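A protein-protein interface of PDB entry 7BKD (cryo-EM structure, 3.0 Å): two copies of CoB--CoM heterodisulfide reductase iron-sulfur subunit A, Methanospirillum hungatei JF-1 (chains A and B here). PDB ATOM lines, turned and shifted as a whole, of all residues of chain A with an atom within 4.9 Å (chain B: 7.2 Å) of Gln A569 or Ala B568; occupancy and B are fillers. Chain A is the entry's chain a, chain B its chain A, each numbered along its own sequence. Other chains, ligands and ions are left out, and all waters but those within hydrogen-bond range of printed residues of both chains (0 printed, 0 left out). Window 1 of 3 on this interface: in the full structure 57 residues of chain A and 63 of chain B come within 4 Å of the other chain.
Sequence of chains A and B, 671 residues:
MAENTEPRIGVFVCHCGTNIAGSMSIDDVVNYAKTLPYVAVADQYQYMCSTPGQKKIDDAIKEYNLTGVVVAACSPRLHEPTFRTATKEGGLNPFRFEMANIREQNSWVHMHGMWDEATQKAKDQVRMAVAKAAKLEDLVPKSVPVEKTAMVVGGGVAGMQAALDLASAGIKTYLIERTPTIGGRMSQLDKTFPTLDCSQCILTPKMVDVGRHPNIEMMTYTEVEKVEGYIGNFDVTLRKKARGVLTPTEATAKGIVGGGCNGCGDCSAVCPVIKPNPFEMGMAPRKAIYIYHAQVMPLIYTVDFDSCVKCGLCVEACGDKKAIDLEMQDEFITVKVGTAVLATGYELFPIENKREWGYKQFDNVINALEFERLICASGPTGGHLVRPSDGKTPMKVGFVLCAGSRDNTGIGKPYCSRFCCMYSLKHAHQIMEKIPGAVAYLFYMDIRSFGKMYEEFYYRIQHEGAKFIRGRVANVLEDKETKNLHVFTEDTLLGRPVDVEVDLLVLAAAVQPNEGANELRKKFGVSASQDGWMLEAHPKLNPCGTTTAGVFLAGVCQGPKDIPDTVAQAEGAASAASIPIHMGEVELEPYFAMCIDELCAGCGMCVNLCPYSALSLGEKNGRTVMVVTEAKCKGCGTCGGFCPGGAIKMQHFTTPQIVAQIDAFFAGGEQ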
ATOM      1  N   PRO A 543      13.904  14.026  32.291  1.00  0.00           N
ATOM      2  CA  PRO A 543      13.247  13.215  31.258  1.00  0.00           C
ATOM      3  C   PRO A 543      13.125  11.742  31.605  1.00  0.00           C
ATOM      4  O   PRO A 543      12.413  11.019  30.896  1.00  0.00           O
ATOM      5  CB  PRO A 543      14.151  13.415  30.037  1.00  0.00           C
ATOM      6  CG  PRO A 543      15.499  13.655  30.617  1.00  0.00           C
ATOM      7  CD  PRO A 543      15.296  14.357  31.934  1.00  0.00           C
ATOM      8  N   CYS A 544      13.787  11.272  32.660  1.00  0.00           N
ATOM      9  CA  CYS A 544      13.749   9.864  33.031  1.00  0.00           C
ATOM     10  C   CYS A 544      12.873   9.585  34.244  1.00  0.00           C
ATOM     11  O   CYS A 544      12.197   8.554  34.289  1.00  0.00           O
ATOM     12  CB  CYS A 544      15.166   9.350  33.301  1.00  0.00           C
ATOM     13  SG  CYS A 544      16.219   9.271  31.837  1.00  0.00           S
ATOM     14  N   LEU A 553      11.798   5.990  33.899  1.00  0.00           N
ATOM     15  CA  LEU A 553      11.486   5.558  32.546  1.00  0.00           C
ATOM     16  C   LEU A 553      12.749   5.485  31.700  1.00  0.00           C
ATOM     17  O   LEU A 553      13.724   6.198  31.943  1.00  0.00           O
ATOM     18  CB  LEU A 553      10.485   6.508  31.888  1.00  0.00           C
ATOM     19  CG  LEU A 553       9.171   6.741  32.628  1.00  0.00           C
ATOM     20  CD1 LEU A 553       8.350   7.810  31.932  1.00  0.00           C
ATOM     21  CD2 LEU A 553       8.389   5.445  32.750  1.00  0.00           C
ATOM     22  N   ALA A 554      12.716   4.616  30.692  1.00  0.00           N
ATOM     23  CA  ALA A 554      13.838   4.477  29.773  1.00  0.00           C
ATOM     24  C   ALA A 554      13.335   3.926  28.449  1.00  0.00           C
ATOM     25  O   ALA A 554      12.632   2.913  28.426  1.00  0.00           O
ATOM     26  CB  ALA A 554      14.917   3.562  30.357  1.00  0.00           C
ATOM     27  N   GLY A 555      13.695   4.588  27.358  1.00  0.00           N
ATOM     28  CA  GLY A 555      13.413   4.092  26.028  1.00  0.00           C
ATOM     29  C   GLY A 555      12.142   4.646  25.418  1.00  0.00           C
ATOM     30  O   GLY A 555      11.547   5.621  25.884  1.00  0.00           O
ATOM     31  N   GLN A 558       8.825   6.088  26.868  1.00  0.00           N
ATOM     32  CA  GLN A 558       8.653   7.505  27.152  1.00  0.00           C
ATOM     33  C   GLN A 558       8.388   8.329  25.897  1.00  0.00           C
ATOM     34  O   GLN A 558       8.045   9.511  26.005  1.00  0.00           O
ATOM     35  CB  GLN A 558       9.894   8.037  27.879  1.00  0.00           C
ATOM     36  CG  GLN A 558       9.719   9.384  28.545  1.00  0.00           C
ATOM     37  CD  GLN A 558      10.367  10.501  27.756  1.00  0.00           C
ATOM     38  OE1 GLN A 558      11.275  10.266  26.961  1.00  0.00           O
ATOM     39  NE2 GLN A 558       9.900  11.723  27.966  1.00  0.00           N
ATOM     40  N   LYS A 561      12.230   7.142  19.940  1.00  0.00           N
ATOM     41  CA  LYS A 561      13.628   7.549  19.960  1.00  0.00           C
ATOM     42  C   LYS A 561      14.438   6.607  19.086  1.00  0.00           C
ATOM     43  O   LYS A 561      14.000   5.504  18.753  1.00  0.00           O
ATOM     44  CB  LYS A 561      14.216   7.543  21.378  1.00  0.00           C
ATOM     45  CG  LYS A 561      13.649   8.579  22.324  1.00  0.00           C
ATOM     46  CD  LYS A 561      14.195   8.385  23.723  1.00  0.00           C
ATOM     47  CE  LYS A 561      13.410   9.195  24.731  1.00  0.00           C
ATOM     48  NZ  LYS A 561      12.040   8.645  24.918  1.00  0.00           N
ATOM     49  N   ASP A 565      19.750   7.402  21.424  1.00  0.00           N
ATOM     50  CA  ASP A 565      18.964   8.163  22.388  1.00  0.00           C
ATOM     51  C   ASP A 565      18.341   7.243  23.428  1.00  0.00           C
ATOM     52  O   ASP A 565      18.286   7.579  24.617  1.00  0.00           O
ATOM     53  CB  ASP A 565      17.885   8.967  21.665  1.00  0.00           C
ATOM     54  CG  ASP A 565      18.441  10.192  20.968  1.00  0.00           C
ATOM     55  OD1 ASP A 565      19.606  10.144  20.519  1.00  0.00           O
ATOM     56  OD2 ASP A 565      17.716  11.204  20.870  1.00  0.00           O
ATOM     57  N   THR A 566      17.876   6.072  22.993  1.00  0.00           N
ATOM     58  CA  THR A 566      17.308   5.100  23.919  1.00  0.00           C
ATOM     59  C   THR A 566      18.345   4.631  24.933  1.00  0.00           C
ATOM     60  O   THR A 566      18.053   4.525  26.129  1.00  0.00           O
ATOM     61  CB  THR A 566      16.746   3.917  23.129  1.00  0.00           C
ATOM     62  OG1 THR A 566      15.566   4.328  22.431  1.00  0.00           O
ATOM     63  CG2 THR A 566      16.404   2.770  24.043  1.00  0.00           C
ATOM     64  N   VAL A 567      19.566   4.361  24.475  1.00  0.00           N
ATOM     65  CA  VAL A 567      20.621   3.901  25.371  1.00  0.00           C
ATOM     66  C   VAL A 567      21.017   5.004  26.345  1.00  0.00           C
ATOM     67  O   VAL A 567      21.266   4.747  27.530  1.00  0.00           O
ATOM     68  CB  VAL A 567      21.822   3.398  24.551  1.00  0.00           C
ATOM     69  CG1 VAL A 567      23.061   3.319  25.408  1.00  0.00           C
ATOM     70  CG2 VAL A 567      21.511   2.044  23.948  1.00  0.00           C
ATOM     71  N   ALA A 568      21.088   6.248  25.866  1.00  0.00           N
ATOM     72  CA  ALA A 568      21.386   7.360  26.762  1.00  0.00           C
ATOM     73  C   ALA A 568      20.316   7.502  27.836  1.00  0.00           C
ATOM     74  O   ALA A 568      20.629   7.695  29.018  1.00  0.00           O
ATOM     75  CB  ALA A 568      21.521   8.654  25.961  1.00  0.00           C
ATOM     76  N   GLN A 569      19.045   7.391  27.443  1.00  0.00           N
ATOM     77  CA  GLN A 569      17.959   7.453  28.414  1.00  0.00           C
ATOM     78  C   GLN A 569      18.048   6.305  29.410  1.00  0.00           C
ATOM     79  O   GLN A 569      17.790   6.489  30.604  1.00  0.00           O
ATOM     80  CB  GLN A 569      16.614   7.427  27.691  1.00  0.00           C
ATOM     81  CG  GLN A 569      16.045   8.794  27.386  1.00  0.00           C
ATOM     82  CD  GLN A 569      15.161   9.314  28.495  1.00  0.00           C
ATOM     83  OE1 GLN A 569      15.369  10.413  29.007  1.00  0.00           O
ATOM     84  NE2 GLN A 569      14.167   8.522  28.879  1.00  0.00           N
ATOM     85  N   ALA A 570      18.401   5.110  28.932  1.00  0.00           N
ATOM     86  CA  ALA A 570      18.519   3.955  29.817  1.00  0.00           C
ATOM     87  C   ALA A 570      19.617   4.156  30.850  1.00  0.00           C
ATOM     88  O   ALA A 570      19.425   3.862  32.036  1.00  0.00           O
ATOM     89  CB  ALA A 570      18.782   2.697  28.994  1.00  0.00           C
ATOM     90  N   GLU A 571      20.777   4.652  30.420  1.00  0.00           N
ATOM     91  CA  GLU A 571      21.859   4.916  31.362  1.00  0.00           C
ATOM     92  C   GLU A 571      21.470   5.996  32.365  1.00  0.00           C
ATOM     93  O   GLU A 571      21.779   5.887  33.558  1.00  0.00           O
ATOM     94  CB  GLU A 571      23.128   5.313  30.614  1.00  0.00           C
ATOM     95  CG  GLU A 571      23.742   4.209  29.786  1.00  0.00           C
ATOM     96  CD  GLU A 571      25.109   4.583  29.251  1.00  0.00           C
ATOM     97  OE1 GLU A 571      25.906   5.171  30.012  1.00  0.00           O
ATOM     98  OE2 GLU A 571      25.387   4.291  28.068  1.00  0.00           O
ATOM     99  N   GLY A 572      20.798   7.052  31.900  1.00  0.00           N
ATOM    100  CA  GLY A 572      20.341   8.079  32.822  1.00  0.00           C
ATOM    101  C   GLY A 572      19.366   7.544  33.854  1.00  0.00           C
ATOM    102  O   GLY A 572      19.450   7.881  35.039  1.00  0.00           O
ATOM    103  N   ALA A 573      18.430   6.701  33.417  1.00  0.00           N
ATOM    104  CA  ALA A 573      17.479   6.096  34.343  1.00  0.00           C
ATOM    105  C   ALA A 573      18.183   5.185  35.337  1.00  0.00           C
ATOM    106  O   ALA A 573      17.824   5.149  36.519  1.00  0.00           O
ATOM    107  CB  ALA A 573      16.416   5.321  33.567  1.00  0.00           C
ATOM    108  N   GLN B 161      24.210  18.891  35.205  1.00  0.00           N
ATOM    109  CA  GLN B 161      23.495  17.649  35.476  1.00  0.00           C
ATOM    110  C   GLN B 161      24.459  16.521  35.810  1.00  0.00           C
ATOM    111  O   GLN B 161      24.219  15.749  36.745  1.00  0.00           O
ATOM    112  CB  GLN B 161      22.625  17.276  34.276  1.00  0.00           C
ATOM    113  CG  GLN B 161      21.602  16.163  34.510  1.00  0.00           C
ATOM    114  CD  GLN B 161      20.873  16.259  35.842  1.00  0.00           C
ATOM    115  OE1 GLN B 161      21.423  15.948  36.898  1.00  0.00           O
ATOM    116  NE2 GLN B 161      19.622  16.696  35.793  1.00  0.00           N
ATOM    117  N   PRO B 543      26.780   5.832  23.243  1.00  0.00           N
ATOM    118  CA  PRO B 543      26.786   7.256  22.880  1.00  0.00           C
ATOM    119  C   PRO B 543      27.562   8.125  23.850  1.00  0.00           C
ATOM    120  O   PRO B 543      27.931   9.248  23.487  1.00  0.00           O
ATOM    121  CB  PRO B 543      25.298   7.620  22.876  1.00  0.00           C
ATOM    122  CG  PRO B 543      24.692   6.676  23.845  1.00  0.00           C
ATOM    123  CD  PRO B 543      25.457   5.391  23.713  1.00  0.00           C
ATOM    124  N   CYS B 544      27.821   7.650  25.066  1.00  0.00           N
ATOM    125  CA  CYS B 544      28.487   8.461  26.073  1.00  0.00           C
ATOM    126  C   CYS B 544      29.992   8.246  26.111  1.00  0.00           C
ATOM    127  O   CYS B 544      30.731   9.163  26.486  1.00  0.00           O
ATOM    128  CB  CYS B 544      27.899   8.162  27.455  1.00  0.00           C
ATOM    129  SG  CYS B 544      26.094   8.090  27.496  1.00  0.00           S
ATOM    130  N   ASP B 562      18.640  18.802  21.928  1.00  0.00           N
ATOM    131  CA  ASP B 562      17.730  19.564  22.765  1.00  0.00           C
ATOM    132  C   ASP B 562      18.166  19.477  24.225  1.00  0.00           C
ATOM    133  O   ASP B 562      19.036  18.688  24.594  1.00  0.00           O
ATOM    134  CB  ASP B 562      16.302  19.045  22.615  1.00  0.00           C
ATOM    135  CG  ASP B 562      15.720  19.331  21.253  1.00  0.00           C
ATOM    136  OD1 ASP B 562      16.119  20.340  20.636  1.00  0.00           O
ATOM    137  OD2 ASP B 562      14.863  18.546  20.797  1.00  0.00           O
ATOM    138  N   ILE B 563      17.547  20.307  25.065  1.00  0.00           N
ATOM    139  CA  ILE B 563      17.832  20.255  26.500  1.00  0.00           C
ATOM    140  C   ILE B 563      17.481  18.902  27.111  1.00  0.00           C
ATOM    141  O   ILE B 563      18.298  18.369  27.879  1.00  0.00           O
ATOM    142  CB  ILE B 563      17.150  21.431  27.220  1.00  0.00           C
ATOM    143  CG1 ILE B 563      17.875  22.739  26.896  1.00  0.00           C
ATOM    144  CG2 ILE B 563      17.108  21.199  28.724  1.00  0.00           C
ATOM    145  CD1 ILE B 563      17.081  23.976  27.234  1.00  0.00           C
ATOM    146  N   PRO B 564      16.311  18.302  26.843  1.00  0.00           N
ATOM    147  CA  PRO B 564      16.047  16.974  27.431  1.00  0.00           C
ATOM    148  C   PRO B 564      17.015  15.899  26.968  1.00  0.00           C
ATOM    149  O   PRO B 564      17.476  15.090  27.785  1.00  0.00           O
ATOM    150  CB  PRO B 564      14.608  16.675  26.984  1.00  0.00           C
ATOM    151  CG  PRO B 564      14.376  17.562  25.818  1.00  0.00           C
ATOM    152  CD  PRO B 564      15.132  18.806  26.120  1.00  0.00           C
ATOM    153  N   ASP B 565      17.338  15.865  25.676  1.00  0.00           N
ATOM    154  CA  ASP B 565      18.314  14.898  25.188  1.00  0.00           C
ATOM    155  C   ASP B 565      19.689  15.166  25.784  1.00  0.00           C
ATOM    156  O   ASP B 565      20.423  14.230  26.121  1.00  0.00           O
ATOM    157  CB  ASP B 565      18.370  14.932  23.663  1.00  0.00           C
ATOM    158  CG  ASP B 565      17.292  14.078  23.022  1.00  0.00           C
ATOM    159  OD1 ASP B 565      16.492  13.473  23.767  1.00  0.00           O
ATOM    160  OD2 ASP B 565      17.246  14.011  21.776  1.00  0.00           O
ATOM    161  N   THR B 566      20.047  16.442  25.929  1.00  0.00           N
ATOM    162  CA  THR B 566      21.312  16.795  26.561  1.00  0.00           C
ATOM    163  C   THR B 566      21.365  16.301  28.001  1.00  0.00           C
ATOM    164  O   THR B 566      22.386  15.768  28.444  1.00  0.00           O
ATOM    165  CB  THR B 566      21.516  18.309  26.498  1.00  0.00           C
ATOM    166  OG1 THR B 566      21.853  18.691  25.159  1.00  0.00           O
ATOM    167  CG2 THR B 566      22.617  18.749  27.431  1.00  0.00           C
ATOM    168  N   VAL B 567      20.269  16.458  28.744  1.00  0.00           N
ATOM    169  CA  VAL B 567      20.244  16.029  30.138  1.00  0.00           C
ATOM    170  C   VAL B 567      20.312  14.510  30.232  1.00  0.00           C
ATOM    171  O   VAL B 567      20.993  13.960  31.107  1.00  0.00           O
ATOM    172  CB  VAL B 567      18.996  16.591  30.843  1.00  0.00           C
ATOM    173  CG1 VAL B 567      18.772  15.896  32.176  1.00  0.00           C
ATOM    174  CG2 VAL B 567      19.139  18.086  31.046  1.00  0.00           C
ATOM    175  N   ALA B 568      19.611  13.808  29.340  1.00  0.00           N
ATOM    176  CA  ALA B 568      19.699  12.352  29.327  1.00  0.00           C
ATOM    177  C   ALA B 568      21.121  11.892  29.039  1.00  0.00           C
ATOM    178  O   ALA B 568      21.639  10.982  29.699  1.00  0.00           O
ATOM    179  CB  ALA B 568      18.728  11.778  28.297  1.00  0.00           C
ATOM    180  N   GLN B 569      21.774  12.525  28.062  1.00  0.00           N
ATOM    181  CA  GLN B 569      23.159  12.200  27.746  1.00  0.00           C
ATOM    182  C   GLN B 569      24.075  12.474  28.933  1.00  0.00           C
ATOM    183  O   GLN B 569      24.974  11.680  29.231  1.00  0.00           O
ATOM    184  CB  GLN B 569      23.599  13.005  26.524  1.00  0.00           C
ATOM    185  CG  GLN B 569      25.074  12.933  26.205  1.00  0.00           C
ATOM    186  CD  GLN B 569      25.377  11.939  25.110  1.00  0.00           C
ATOM    187  OE1 GLN B 569      24.618  11.001  24.878  1.00  0.00           O
ATOM    188  NE2 GLN B 569      26.491  12.145  24.419  1.00  0.00           N
ATOM    189  N   ALA B 570      23.862  13.598  29.619  1.00  0.00           N
ATOM    190  CA  ALA B 570      24.694  13.945  30.766  1.00  0.00           C
ATOM    191  C   ALA B 570      24.531  12.940  31.896  1.00  0.00           C
ATOM    192  O   ALA B 570      25.516  12.538  32.525  1.00  0.00           O
ATOM    193  CB  ALA B 570      24.354  15.351  31.250  1.00  0.00           C
ATOM    194  N   GLU B 571      23.295  12.527  32.176  1.00  0.00           N
ATOM    195  CA  GLU B 571      23.074  11.534  33.221  1.00  0.00           C
ATOM    196  C   GLU B 571      23.683  10.190  32.845  1.00  0.00           C
ATOM    197  O   GLU B 571      24.251   9.497  33.699  1.00  0.00           O
ATOM    198  CB  GLU B 571      21.582  11.395  33.505  1.00  0.00           C
ATOM    199  CG  GLU B 571      21.083  12.347  34.568  1.00  0.00           C
ATOM    200  CD  GLU B 571      19.639  12.741  34.363  1.00  0.00           C
ATOM    201  OE1 GLU B 571      19.039  12.301  33.361  1.00  0.00           O
ATOM    202  OE2 GLU B 571      19.102  13.492  35.204  1.00  0.00           O
ATOM    203  N   GLY B 572      23.582   9.802  31.572  1.00  0.00           N
ATOM    204  CA  GLY B 572      24.227   8.574  31.140  1.00  0.00           C
ATOM    205  C   GLY B 572      25.734   8.624  31.293  1.00  0.00           C
ATOM    206  O   GLY B 572      26.359   7.658  31.742  1.00  0.00           O
ATOM    207  N   ALA B 573      26.339   9.753  30.920  1.00  0.00           N
ATOM    208  CA  ALA B 573      27.777   9.916  31.091  1.00  0.00           C
ATOM    209  C   ALA B 573      28.162   9.876  32.562  1.00  0.00           C
ATOM    210  O   ALA B 573      29.188   9.290  32.928  1.00  0.00           O
ATOM    211  CB  ALA B 573      28.239  11.225  30.451  1.00  0.00           C
ATOM    212  N   ALA B 574      27.352  10.496  33.421  1.00  0.00           N
ATOM    213  CA  ALA B 574      27.625  10.460  34.853  1.00  0.00           C
ATOM    214  C   ALA B 574      27.582   9.035  35.381  1.00  0.00           C
ATOM    215  O   ALA B 574      28.430   8.638  36.187  1.00  0.00           O
ATOM    216  CB  ALA B 574      26.628  11.341  35.600  1.00  0.00           C
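OD2 of Asp B565 lies close to OD2 of Asp A565. The side-chain carboxylate (OE1) of Glu A571 lies close to the backbone carbonyl oxygen (O) of Gly B572 (3.1 Å).
OE2 of Glu B571 is in hydrogen-bond range of NE2 of Gln B161, 3.3 Å away. The side-chain amide nitrogen of Gln B569 sits at hydrogen-bond distance from the backbone carbonyl oxygen of Pro B543 (3.4 Å). SG of Cys A544 lies within hydrogen-bond range of OE1 of Gln A569, 3.2 Å away.
Among the printed residues, merely in contact across the chains: Ala A568 with Ala B568 (3.5 Å), Val A567 with Pro B543 (3.6 Å), Gly A572 with Glu B571 (3.6 Å), Gln A569 with Ala B568 (3.7 Å), Pro A543 with Pro B564 (3.7 Å), Pro A543 with Val B567 (3.8 Å), Gly A572 with Gly B572 (3.8 Å) and Glu A571 with Cys B544 (3.9 Å).
Gln A569 touches just one residue of chain B: Ala B568. Ala B568 touches just these residues of chain A: Ala A568 and Gln A569. Of chain B, only Ala B568 comes within 4 Å of Ala A568. Of the printed residues of chain B, Glu A571 touches Cys B544 (3.9 Å) and Gly B572 (3.1 Å). Of the printed residues of chain B, Pro A543 touches Pro B564 (3.7 Å) and Val B567 (3.8 Å). Of the printed residues of chain B, Val A567 touches Pro B543. Cys A544 touches none of the printed residues of chain B.
Hydrophobic or aromatic side chains of chain A that line the printed part of chain B: Pro A543 and Val A567. Of the 16 printed residues of chain B, 8 touch a printed residue of chain A. Along chain B the printed residues that touch a printed residue of chain A span positions 543 to 572. Among the printed residues, no Asp or Glu carboxylate lies within 4 Å of a Lys or Arg side-chain nitrogen of the other chain.
Pro A543 touches Val B567, and with the chains exchanged Val A567 touches Pro B543. Asp B565 touches its own counterpart, Asp A565. Glu A571 touches Cys B544, but with the chains exchanged Cys A544 does not touch Glu B571 (4.4 Å). Glu A571 touches Gly B572, and with the chains exchanged Gly A572 touches Glu B571.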
